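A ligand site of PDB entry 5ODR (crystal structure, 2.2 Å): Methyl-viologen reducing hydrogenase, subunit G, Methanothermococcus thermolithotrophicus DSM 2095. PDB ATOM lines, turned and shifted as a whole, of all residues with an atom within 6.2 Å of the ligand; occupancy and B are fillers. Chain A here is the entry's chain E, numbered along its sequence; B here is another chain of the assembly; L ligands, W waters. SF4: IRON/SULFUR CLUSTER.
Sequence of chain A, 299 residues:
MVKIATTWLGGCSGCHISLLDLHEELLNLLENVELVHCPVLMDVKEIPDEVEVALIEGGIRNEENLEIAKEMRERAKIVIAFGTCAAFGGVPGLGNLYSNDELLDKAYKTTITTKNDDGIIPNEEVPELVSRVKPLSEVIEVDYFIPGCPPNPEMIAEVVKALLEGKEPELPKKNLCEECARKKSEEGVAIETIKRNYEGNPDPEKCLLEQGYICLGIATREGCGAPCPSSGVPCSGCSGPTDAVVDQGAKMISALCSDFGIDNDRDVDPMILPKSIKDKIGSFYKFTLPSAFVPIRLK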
ATOM      1  N   GLY A  10      30.452 -17.645 -21.078  1.00  0.00           N
ATOM      2  CA  GLY A  10      30.932 -16.679 -22.059  1.00  0.00           C
ATOM      3  C   GLY A  10      30.282 -16.754 -23.433  1.00  0.00           C
ATOM      4  O   GLY A  10      30.947 -16.470 -24.428  1.00  0.00           O
ATOM      5  N   GLY A  11      29.005 -17.116 -23.477  1.00  0.00           N
ATOM      6  CA  GLY A  11      28.267 -17.226 -24.732  1.00  0.00           C
ATOM      7  C   GLY A  11      27.378 -16.029 -25.016  1.00  0.00           C
ATOM      8  O   GLY A  11      27.654 -14.921 -24.546  1.00  0.00           O
ATOM      9  N   CYS A  12      26.295 -16.251 -25.792  1.00  0.00           N
ATOM     10  CA  CYS A  12      25.349 -15.200 -26.175  1.00  0.00           C
ATOM     11  C   CYS A  12      23.890 -15.480 -25.835  1.00  0.00           C
ATOM     12  O   CYS A  12      23.049 -14.658 -26.198  1.00  0.00           O
ATOM     13  CB  CYS A  12      25.506 -14.963 -27.675  1.00  0.00           C
ATOM     14  SG  CYS A  12      24.666 -16.191 -28.704  1.00  0.00           S
ATOM     15  N   SER A  13      23.570 -16.615 -25.180  1.00  0.00           N
ATOM     16  CA  SER A  13      22.195 -17.045 -24.819  1.00  0.00           C
ATOM     17  C   SER A  13      21.511 -17.819 -25.965  1.00  0.00           C
ATOM     18  O   SER A  13      20.437 -18.368 -25.763  1.00  0.00           O
ATOM     19  CB  SER A  13      21.314 -15.869 -24.393  1.00  0.00           C
ATOM     20  OG  SER A  13      20.605 -15.298 -25.482  1.00  0.00           O
ATOM     21  N   GLY A  14      22.133 -17.855 -27.149  1.00  0.00           N
ATOM     22  CA  GLY A  14      21.595 -18.541 -28.323  1.00  0.00           C
ATOM     23  C   GLY A  14      21.288 -20.003 -28.149  1.00  0.00           C
ATOM     24  O   GLY A  14      20.349 -20.518 -28.766  1.00  0.00           O
ATOM     25  N   CYS A  15      22.054 -20.709 -27.309  1.00  0.00           N
ATOM     26  CA  CYS A  15      21.797 -22.138 -27.087  1.00  0.00           C
ATOM     27  C   CYS A  15      20.525 -22.281 -26.255  1.00  0.00           C
ATOM     28  O   CYS A  15      19.720 -23.177 -26.525  1.00  0.00           O
ATOM     29  CB  CYS A  15      22.994 -22.814 -26.424  1.00  0.00           C
ATOM     30  SG  CYS A  15      24.445 -22.935 -27.502  1.00  0.00           S
ATOM     31  N   HIS A  16      20.319 -21.396 -25.282  1.00  0.00           N
ATOM     32  CA  HIS A  16      19.112 -21.409 -24.456  1.00  0.00           C
ATOM     33  C   HIS A  16      17.915 -21.068 -25.365  1.00  0.00           C
ATOM     34  O   HIS A  16      16.857 -21.670 -25.222  1.00  0.00           O
ATOM     35  CB  HIS A  16      19.181 -20.384 -23.310  1.00  0.00           C
ATOM     36  CG  HIS A  16      19.922 -20.868 -22.099  1.00  0.00           C
ATOM     37  ND1 HIS A  16      21.278 -21.101 -22.133  1.00  0.00           N
ATOM     38  CD2 HIS A  16      19.472 -21.119 -20.854  1.00  0.00           C
ATOM     39  CE1 HIS A  16      21.611 -21.495 -20.920  1.00  0.00           C
ATOM     40  NE2 HIS A  16      20.549 -21.520 -20.116  1.00  0.00           N
ATOM     41  N   GLU A  57      26.107 -23.457 -21.012  1.00  0.00           N
ATOM     42  CA  GLU A  57      26.340 -22.735 -22.257  1.00  0.00           C
ATOM     43  C   GLU A  57      27.549 -21.817 -22.117  1.00  0.00           C
ATOM     44  O   GLU A  57      27.815 -21.326 -21.028  1.00  0.00           O
ATOM     45  CB  GLU A  57      25.099 -21.903 -22.619  1.00  0.00           C
ATOM     46  CG  GLU A  57      25.311 -20.893 -23.726  1.00  0.00           C
ATOM     47  CD  GLU A  57      24.220 -19.844 -23.787  1.00  0.00           C
ATOM     48  OE1 GLU A  57      24.411 -18.740 -23.213  1.00  0.00           O
ATOM     49  OE2 GLU A  57      23.159 -20.135 -24.362  1.00  0.00           O
ATOM     50  N   GLY A  58      28.258 -21.588 -23.218  1.00  0.00           N
ATOM     51  CA  GLY A  58      29.418 -20.709 -23.240  1.00  0.00           C
ATOM     52  C   GLY A  58      30.720 -21.252 -22.714  1.00  0.00           C
ATOM     53  O   GLY A  58      30.729 -22.199 -21.916  1.00  0.00           O
ATOM     54  N   PHE A  82      27.049 -27.241 -23.487  1.00  0.00           N
ATOM     55  CA  PHE A  82      25.947 -26.848 -24.357  1.00  0.00           C
ATOM     56  C   PHE A  82      26.332 -25.836 -25.432  1.00  0.00           C
ATOM     57  O   PHE A  82      26.442 -24.649 -25.153  1.00  0.00           O
ATOM     58  CB  PHE A  82      24.794 -26.298 -23.490  1.00  0.00           C
ATOM     59  CG  PHE A  82      23.462 -26.115 -24.187  1.00  0.00           C
ATOM     60  CD1 PHE A  82      23.184 -26.752 -25.385  1.00  0.00           C
ATOM     61  CD2 PHE A  82      22.473 -25.312 -23.633  1.00  0.00           C
ATOM     62  CE1 PHE A  82      21.964 -26.586 -26.015  1.00  0.00           C
ATOM     63  CE2 PHE A  82      21.253 -25.146 -24.264  1.00  0.00           C
ATOM     64  CZ  PHE A  82      21.002 -25.783 -25.457  1.00  0.00           C
ATOM     65  N   GLY A  83      26.506 -26.325 -26.653  1.00  0.00           N
ATOM     66  CA  GLY A  83      26.857 -25.466 -27.781  1.00  0.00           C
ATOM     67  C   GLY A  83      28.338 -25.383 -28.065  1.00  0.00           C
ATOM     68  O   GLY A  83      29.181 -25.810 -27.273  1.00  0.00           O
ATOM     69  N   THR A  84      28.645 -24.806 -29.220  1.00  0.00           N
ATOM     70  CA  THR A  84      29.996 -24.607 -29.750  1.00  0.00           C
ATOM     71  C   THR A  84      30.894 -23.737 -28.858  1.00  0.00           C
ATOM     72  O   THR A  84      32.098 -23.966 -28.827  1.00  0.00           O
ATOM     73  CB  THR A  84      29.884 -24.065 -31.176  1.00  0.00           C
ATOM     74  OG1 THR A  84      29.530 -25.163 -32.015  1.00  0.00           O
ATOM     75  CG2 THR A  84      31.157 -23.403 -31.686  1.00  0.00           C
ATOM     76  N   CYS A  85      30.329 -22.754 -28.133  1.00  0.00           N
ATOM     77  CA  CYS A  85      31.153 -21.926 -27.271  1.00  0.00           C
ATOM     78  C   CYS A  85      31.705 -22.774 -26.124  1.00  0.00           C
ATOM     79  O   CYS A  85      32.904 -22.761 -25.864  1.00  0.00           O
ATOM     80  CB  CYS A  85      30.383 -20.723 -26.730  1.00  0.00           C
ATOM     81  SG  CYS A  85      30.115 -19.398 -27.943  1.00  0.00           S
ATOM     82  N   ALA A  86      30.833 -23.528 -25.460  1.00  0.00           N
ATOM     83  CA  ALA A  86      31.225 -24.377 -24.343  1.00  0.00           C
ATOM     84  C   ALA A  86      32.103 -25.545 -24.791  1.00  0.00           C
ATOM     85  O   ALA A  86      32.955 -25.993 -24.018  1.00  0.00           O
ATOM     86  CB  ALA A  86      29.993 -24.897 -23.621  1.00  0.00           C
ATOM     87  N   GLY A  90      34.067 -20.934 -29.378  1.00  0.00           N
ATOM     88  CA  GLY A  90      33.189 -20.044 -30.144  1.00  0.00           C
ATOM     89  C   GLY A  90      33.813 -18.760 -30.636  1.00  0.00           C
ATOM     90  O   GLY A  90      35.016 -18.544 -30.516  1.00  0.00           O
ATOM     91  N   VAL A  91      32.958 -17.889 -31.204  1.00  0.00           N
ATOM     92  CA  VAL A  91      33.346 -16.578 -31.745  1.00  0.00           C
ATOM     93  C   VAL A  91      34.096 -15.710 -30.716  1.00  0.00           C
ATOM     94  O   VAL A  91      35.091 -15.080 -31.077  1.00  0.00           O
ATOM     95  CB  VAL A  91      32.119 -15.839 -32.351  1.00  0.00           C
ATOM     96  CG1 VAL A  91      32.425 -14.362 -32.626  1.00  0.00           C
ATOM     97  CG2 VAL A  91      31.644 -16.530 -33.623  1.00  0.00           C
ATOM     98  N   PRO A  92      33.688 -15.668 -29.431  1.00  0.00           N
ATOM     99  CA  PRO A  92      34.432 -14.854 -28.457  1.00  0.00           C
ATOM    100  C   PRO A  92      35.910 -15.241 -28.386  1.00  0.00           C
ATOM    101  O   PRO A  92      36.742 -14.429 -27.994  1.00  0.00           O
ATOM    102  CB  PRO A  92      33.686 -15.110 -27.139  1.00  0.00           C
ATOM    103  CG  PRO A  92      32.300 -15.514 -27.574  1.00  0.00           C
ATOM    104  CD  PRO A  92      32.533 -16.343 -28.797  1.00  0.00           C
ATOM    105  N   GLY A 148      27.250 -27.106 -32.054  1.00  0.00           N
ATOM    106  CA  GLY A 148      26.378 -26.269 -32.859  1.00  0.00           C
ATOM    107  C   GLY A 148      26.310 -24.857 -32.332  1.00  0.00           C
ATOM    108  O   GLY A 148      26.346 -24.639 -31.117  1.00  0.00           O
ATOM    109  N   CYS A 149      26.188 -23.886 -33.247  1.00  0.00           N
ATOM    110  CA  CYS A 149      26.112 -22.484 -32.878  1.00  0.00           C
ATOM    111  C   CYS A 149      24.821 -21.829 -33.381  1.00  0.00           C
ATOM    112  O   CYS A 149      24.863 -21.061 -34.333  1.00  0.00           O
ATOM    113  CB  CYS A 149      27.331 -21.730 -33.365  1.00  0.00           C
ATOM    114  SG  CYS A 149      27.465 -20.052 -32.717  1.00  0.00           S
ATOM    115  N   PRO A 150      23.679 -22.094 -32.754  1.00  0.00           N
ATOM    116  CA  PRO A 150      23.464 -23.003 -31.625  1.00  0.00           C
ATOM    117  C   PRO A 150      23.105 -24.384 -32.156  1.00  0.00           C
ATOM    118  O   PRO A 150      22.845 -24.520 -33.358  1.00  0.00           O
ATOM    119  CB  PRO A 150      22.248 -22.372 -30.929  1.00  0.00           C
ATOM    120  CG  PRO A 150      21.439 -21.814 -32.067  1.00  0.00           C
ATOM    121  CD  PRO A 150      22.406 -21.476 -33.181  1.00  0.00           C
ATOM    122  N   PRO A 151      23.068 -25.420 -31.331  1.00  0.00           N
ATOM    123  CA  PRO A 151      22.677 -26.730 -31.842  1.00  0.00           C
ATOM    124  C   PRO A 151      21.214 -26.691 -32.256  1.00  0.00           C
ATOM    125  O   PRO A 151      20.466 -25.889 -31.698  1.00  0.00           O
ATOM    126  CB  PRO A 151      22.902 -27.665 -30.643  1.00  0.00           C
ATOM    127  CG  PRO A 151      23.740 -26.881 -29.676  1.00  0.00           C
ATOM    128  CD  PRO A 151      23.331 -25.470 -29.883  1.00  0.00           C
ATOM    129  N   PHE A 287      34.892 -20.209 -35.074  1.00  0.00           N
ATOM    130  CA  PHE A 287      34.251 -20.763 -33.881  1.00  0.00           C
ATOM    131  C   PHE A 287      35.068 -21.719 -33.042  1.00  0.00           C
ATOM    132  O   PHE A 287      34.559 -22.193 -32.028  1.00  0.00           O
ATOM    133  CB  PHE A 287      33.016 -21.550 -34.361  1.00  0.00           C
ATOM    134  CG  PHE A 287      32.075 -20.756 -35.223  1.00  0.00           C
ATOM    135  CD1 PHE A 287      32.244 -20.692 -36.597  1.00  0.00           C
ATOM    136  CD2 PHE A 287      31.013 -20.073 -34.658  1.00  0.00           C
ATOM    137  CE1 PHE A 287      31.371 -19.954 -37.382  1.00  0.00           C
ATOM    138  CE2 PHE A 287      30.147 -19.335 -35.450  1.00  0.00           C
ATOM    139  CZ  PHE A 287      30.321 -19.280 -36.802  1.00  0.00           C
ATOM    140  N   ARG B  39      33.019  -9.398 -23.660  1.00  0.00           N
ATOM    141  CA  ARG B  39      33.737 -10.310 -24.567  1.00  0.00           C
ATOM    142  C   ARG B  39      34.745  -9.601 -25.481  1.00  0.00           C
ATOM    143  O   ARG B  39      35.685 -10.248 -25.943  1.00  0.00           O
ATOM    144  CB  ARG B  39      32.747 -11.165 -25.366  1.00  0.00           C
ATOM    145  CG  ARG B  39      32.171 -12.299 -24.504  1.00  0.00           C
ATOM    146  CD  ARG B  39      30.917 -12.892 -25.104  1.00  0.00           C
ATOM    147  NE  ARG B  39      29.847 -11.895 -25.216  1.00  0.00           N
ATOM    148  CZ  ARG B  39      28.795 -11.989 -26.008  1.00  0.00           C
ATOM    149  NH1 ARG B  39      28.633 -13.044 -26.794  1.00  0.00           N
ATOM    150  NH2 ARG B  39      27.891 -11.018 -26.031  1.00  0.00           N
ATOM    151  N   ARG B  59      26.491 -13.393 -33.124  1.00  0.00           N
ATOM    152  CA  ARG B  59      26.958 -14.109 -31.932  1.00  0.00           C
ATOM    153  C   ARG B  59      27.093 -13.209 -30.690  1.00  0.00           C
ATOM    154  O   ARG B  59      27.461 -13.681 -29.626  1.00  0.00           O
ATOM    155  CB  ARG B  59      28.238 -14.917 -32.216  1.00  0.00           C
ATOM    156  CG  ARG B  59      27.941 -16.273 -32.832  1.00  0.00           C
ATOM    157  CD  ARG B  59      27.530 -16.194 -34.296  1.00  0.00           C
ATOM    158  NE  ARG B  59      27.145 -17.513 -34.798  1.00  0.00           N
ATOM    159  CZ  ARG B  59      26.861 -17.774 -36.075  1.00  0.00           C
ATOM    160  NH1 ARG B  59      26.925 -16.824 -36.991  1.00  0.00           N
ATOM    161  NH2 ARG B  59      26.520 -19.006 -36.440  1.00  0.00           N
ATOM    162  N   ILE B  60      26.775 -11.905 -30.836  1.00  0.00           N
ATOM    163  CA  ILE B  60      26.804 -10.980 -29.703  1.00  0.00           C
ATOM    164  C   ILE B  60      25.582 -11.383 -28.858  1.00  0.00           C
ATOM    165  O   ILE B  60      25.632 -11.315 -27.632  1.00  0.00           O
ATOM    166  CB  ILE B  60      26.692  -9.503 -30.152  1.00  0.00           C
ATOM    167  CG1 ILE B  60      28.009  -9.007 -30.760  1.00  0.00           C
ATOM    168  CG2 ILE B  60      26.267  -8.607 -28.988  1.00  0.00           C
ATOM    169  CD1 ILE B  60      27.883  -7.707 -31.515  1.00  0.00           C
ATOM    170  N   CYS B  61      24.470 -11.799 -29.512  1.00  0.00           N
ATOM    171  CA  CYS B  61      23.264 -12.178 -28.780  1.00  0.00           C
ATOM    172  C   CYS B  61      22.370 -13.161 -29.544  1.00  0.00           C
ATOM    173  O   CYS B  61      22.091 -12.976 -30.723  1.00  0.00           O
ATOM    174  CB  CYS B  61      22.480 -10.934 -28.394  1.00  0.00           C
ATOM    175  SG  CYS B  61      20.884 -11.291 -27.632  1.00  0.00           S
ATOM    176  N   GLY B  62      21.929 -14.193 -28.840  1.00  0.00           N
ATOM    177  CA  GLY B  62      21.071 -15.235 -29.389  1.00  0.00           C
ATOM    178  C   GLY B  62      19.602 -14.881 -29.528  1.00  0.00           C
ATOM    179  O   GLY B  62      18.862 -15.617 -30.170  1.00  0.00           O
ATOM    180  N   ILE B 162      18.077 -18.753 -35.804  1.00  0.00           N
ATOM    181  CA  ILE B 162      19.040 -18.124 -34.910  1.00  0.00           C
ATOM    182  C   ILE B 162      20.342 -17.978 -35.702  1.00  0.00           C
ATOM    183  O   ILE B 162      20.881 -18.968 -36.194  1.00  0.00           O
ATOM    184  CB  ILE B 162      19.218 -18.911 -33.583  1.00  0.00           C
ATOM    185  CG1 ILE B 162      17.844 -19.082 -32.886  1.00  0.00           C
ATOM    186  CG2 ILE B 162      20.205 -18.190 -32.663  1.00  0.00           C
ATOM    187  CD1 ILE B 162      17.837 -19.965 -31.665  1.00  0.00           C
ATOM    188  N   HIS B 163      20.831 -16.724 -35.839  1.00  0.00           N
ATOM    189  CA  HIS B 163      22.045 -16.366 -36.576  1.00  0.00           C
ATOM    190  C   HIS B 163      21.792 -16.499 -38.084  1.00  0.00           C
ATOM    191  O   HIS B 163      22.327 -17.378 -38.754  1.00  0.00           O
ATOM    192  CB  HIS B 163      23.285 -17.142 -36.116  1.00  0.00           C
ATOM    193  CG  HIS B 163      23.558 -17.021 -34.648  1.00  0.00           C
ATOM    194  ND1 HIS B 163      23.473 -15.803 -33.998  1.00  0.00           N
ATOM    195  CD2 HIS B 163      23.924 -17.963 -33.743  1.00  0.00           C
ATOM    196  CE1 HIS B 163      23.777 -16.034 -32.734  1.00  0.00           C
ATOM    197  NE2 HIS B 163      24.051 -17.315 -32.532  1.00  0.00           N
HETATM  198 FE1  SF4 L   1      25.472 -20.953 -28.412  1.00  0.00          FE
HETATM  199 FE2  SF4 L   1      25.676 -18.207 -28.730  1.00  0.00          FE
HETATM  200 FE3  SF4 L   1      26.728 -19.827 -30.666  1.00  0.00          FE
HETATM  201 FE4  SF4 L   1      27.898 -19.645 -28.260  1.00  0.00          FE
HETATM  202  S1  SF4 L   1      27.635 -17.926 -29.787  1.00  0.00           S
HETATM  203  S2  SF4 L   1      27.442 -21.588 -29.353  1.00  0.00           S
HETATM  204  S3  SF4 L   1      26.196 -19.413 -26.823  1.00  0.00           S
HETATM  205  S4  SF4 L   1      24.504 -19.653 -30.086  1.00  0.00           S
HETATM  206  O   HOH W   1      29.208 -15.462 -28.138  1.00  0.00           O
HETATM  207  O   HOH W   2      27.648 -22.517 -26.069  1.00  0.00           O
HETATM  208  O   HOH W   3      30.390 -19.455 -31.298  1.00  0.00           O
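NH1 of Arg 39 of chain B sits at hydrogen-bond distance from O of Gly 11 (3.1 Å). OE2 of Glu 57 is in hydrogen-bond range of N of Cys 15. The backbone carbonyl oxygen of Arg 59 of chain B is in hydrogen-bond range of the guanidinium group of Arg 39 of chain B (3.1 Å). O of Cys 12 lies within hydrogen-bond range of N of Gly 62 of chain B. SG of Cys 15 lies close to O of Phe 82, at 3.5 Å. N of Thr 84 lies within hydrogen-bond range of O of Gly 148, at 3.0 Å. O of Cys 149 sits at hydrogen-bond distance from NH2 of Arg 59 of chain B (3.4 Å). OE2 of Glu 57 sits at hydrogen-bond distance from ND1 of His 16.
SG of Cys 15 is bound to FE1 of the ligand. The side-chain sulfur of Cys 85 binds an iron atom (FE4) of the ligand, 2.3 Å away. S2 of the ligand sits close to N of Cys 85, at 3.3 Å. N of Thr 84 lies close to S2 of the ligand, 3.4 Å away. N of Cys 12 lies close to S3 of the ligand, at 3.3 Å. An iron atom (FE2) of the ligand is bound by the side-chain sulfur (SG) of Cys 12 (2.3 Å). The side-chain sulfur of Cys 149 binds an iron atom (FE3) of the ligand, at 2.2 Å. A sulfur (S4) of the ligand lies close to a ring nitrogen (NE2) of His 163 of chain B (3.4 Å).
The backbone carbonyl oxygen of Gly 148 lies close to a sulfur (S2) of the ligand (3.7 Å). A sulfur (S4) of the ligand sits close to the backbone nitrogen of Pro 150 (3.7 Å). CA of Gly 11 touches S3 of the ligand, at 3.7 Å. CA of Gly 14 touches S4 of the ligand (3.6 Å). Glu 57 touches the ligand (CG to S3, 3.5 Å). Arg 59 of chain B touches the ligand. Within 4 Å of the ligand: Gly 11, Cys 12, Gly 14, Cys 15, Glu 57, Thr 84, Cys 85, Gly 148, Cys 149, Pro 150, Arg 59 of chain B and His 163 of chain B.
Water W1 lies within hydrogen-bond range of the guanidinium group of Arg 39 of chain B (2.8 Å), the backbone carbonyl oxygen of Arg 59 of chain B (2.9 Å) and a sulfur (S1) of the ligand (3.4 Å). Water W3 bridges the backbone NH of Val 91 (3.0 Å) and a sulfur (S1) of the ligand (3.5 Å).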
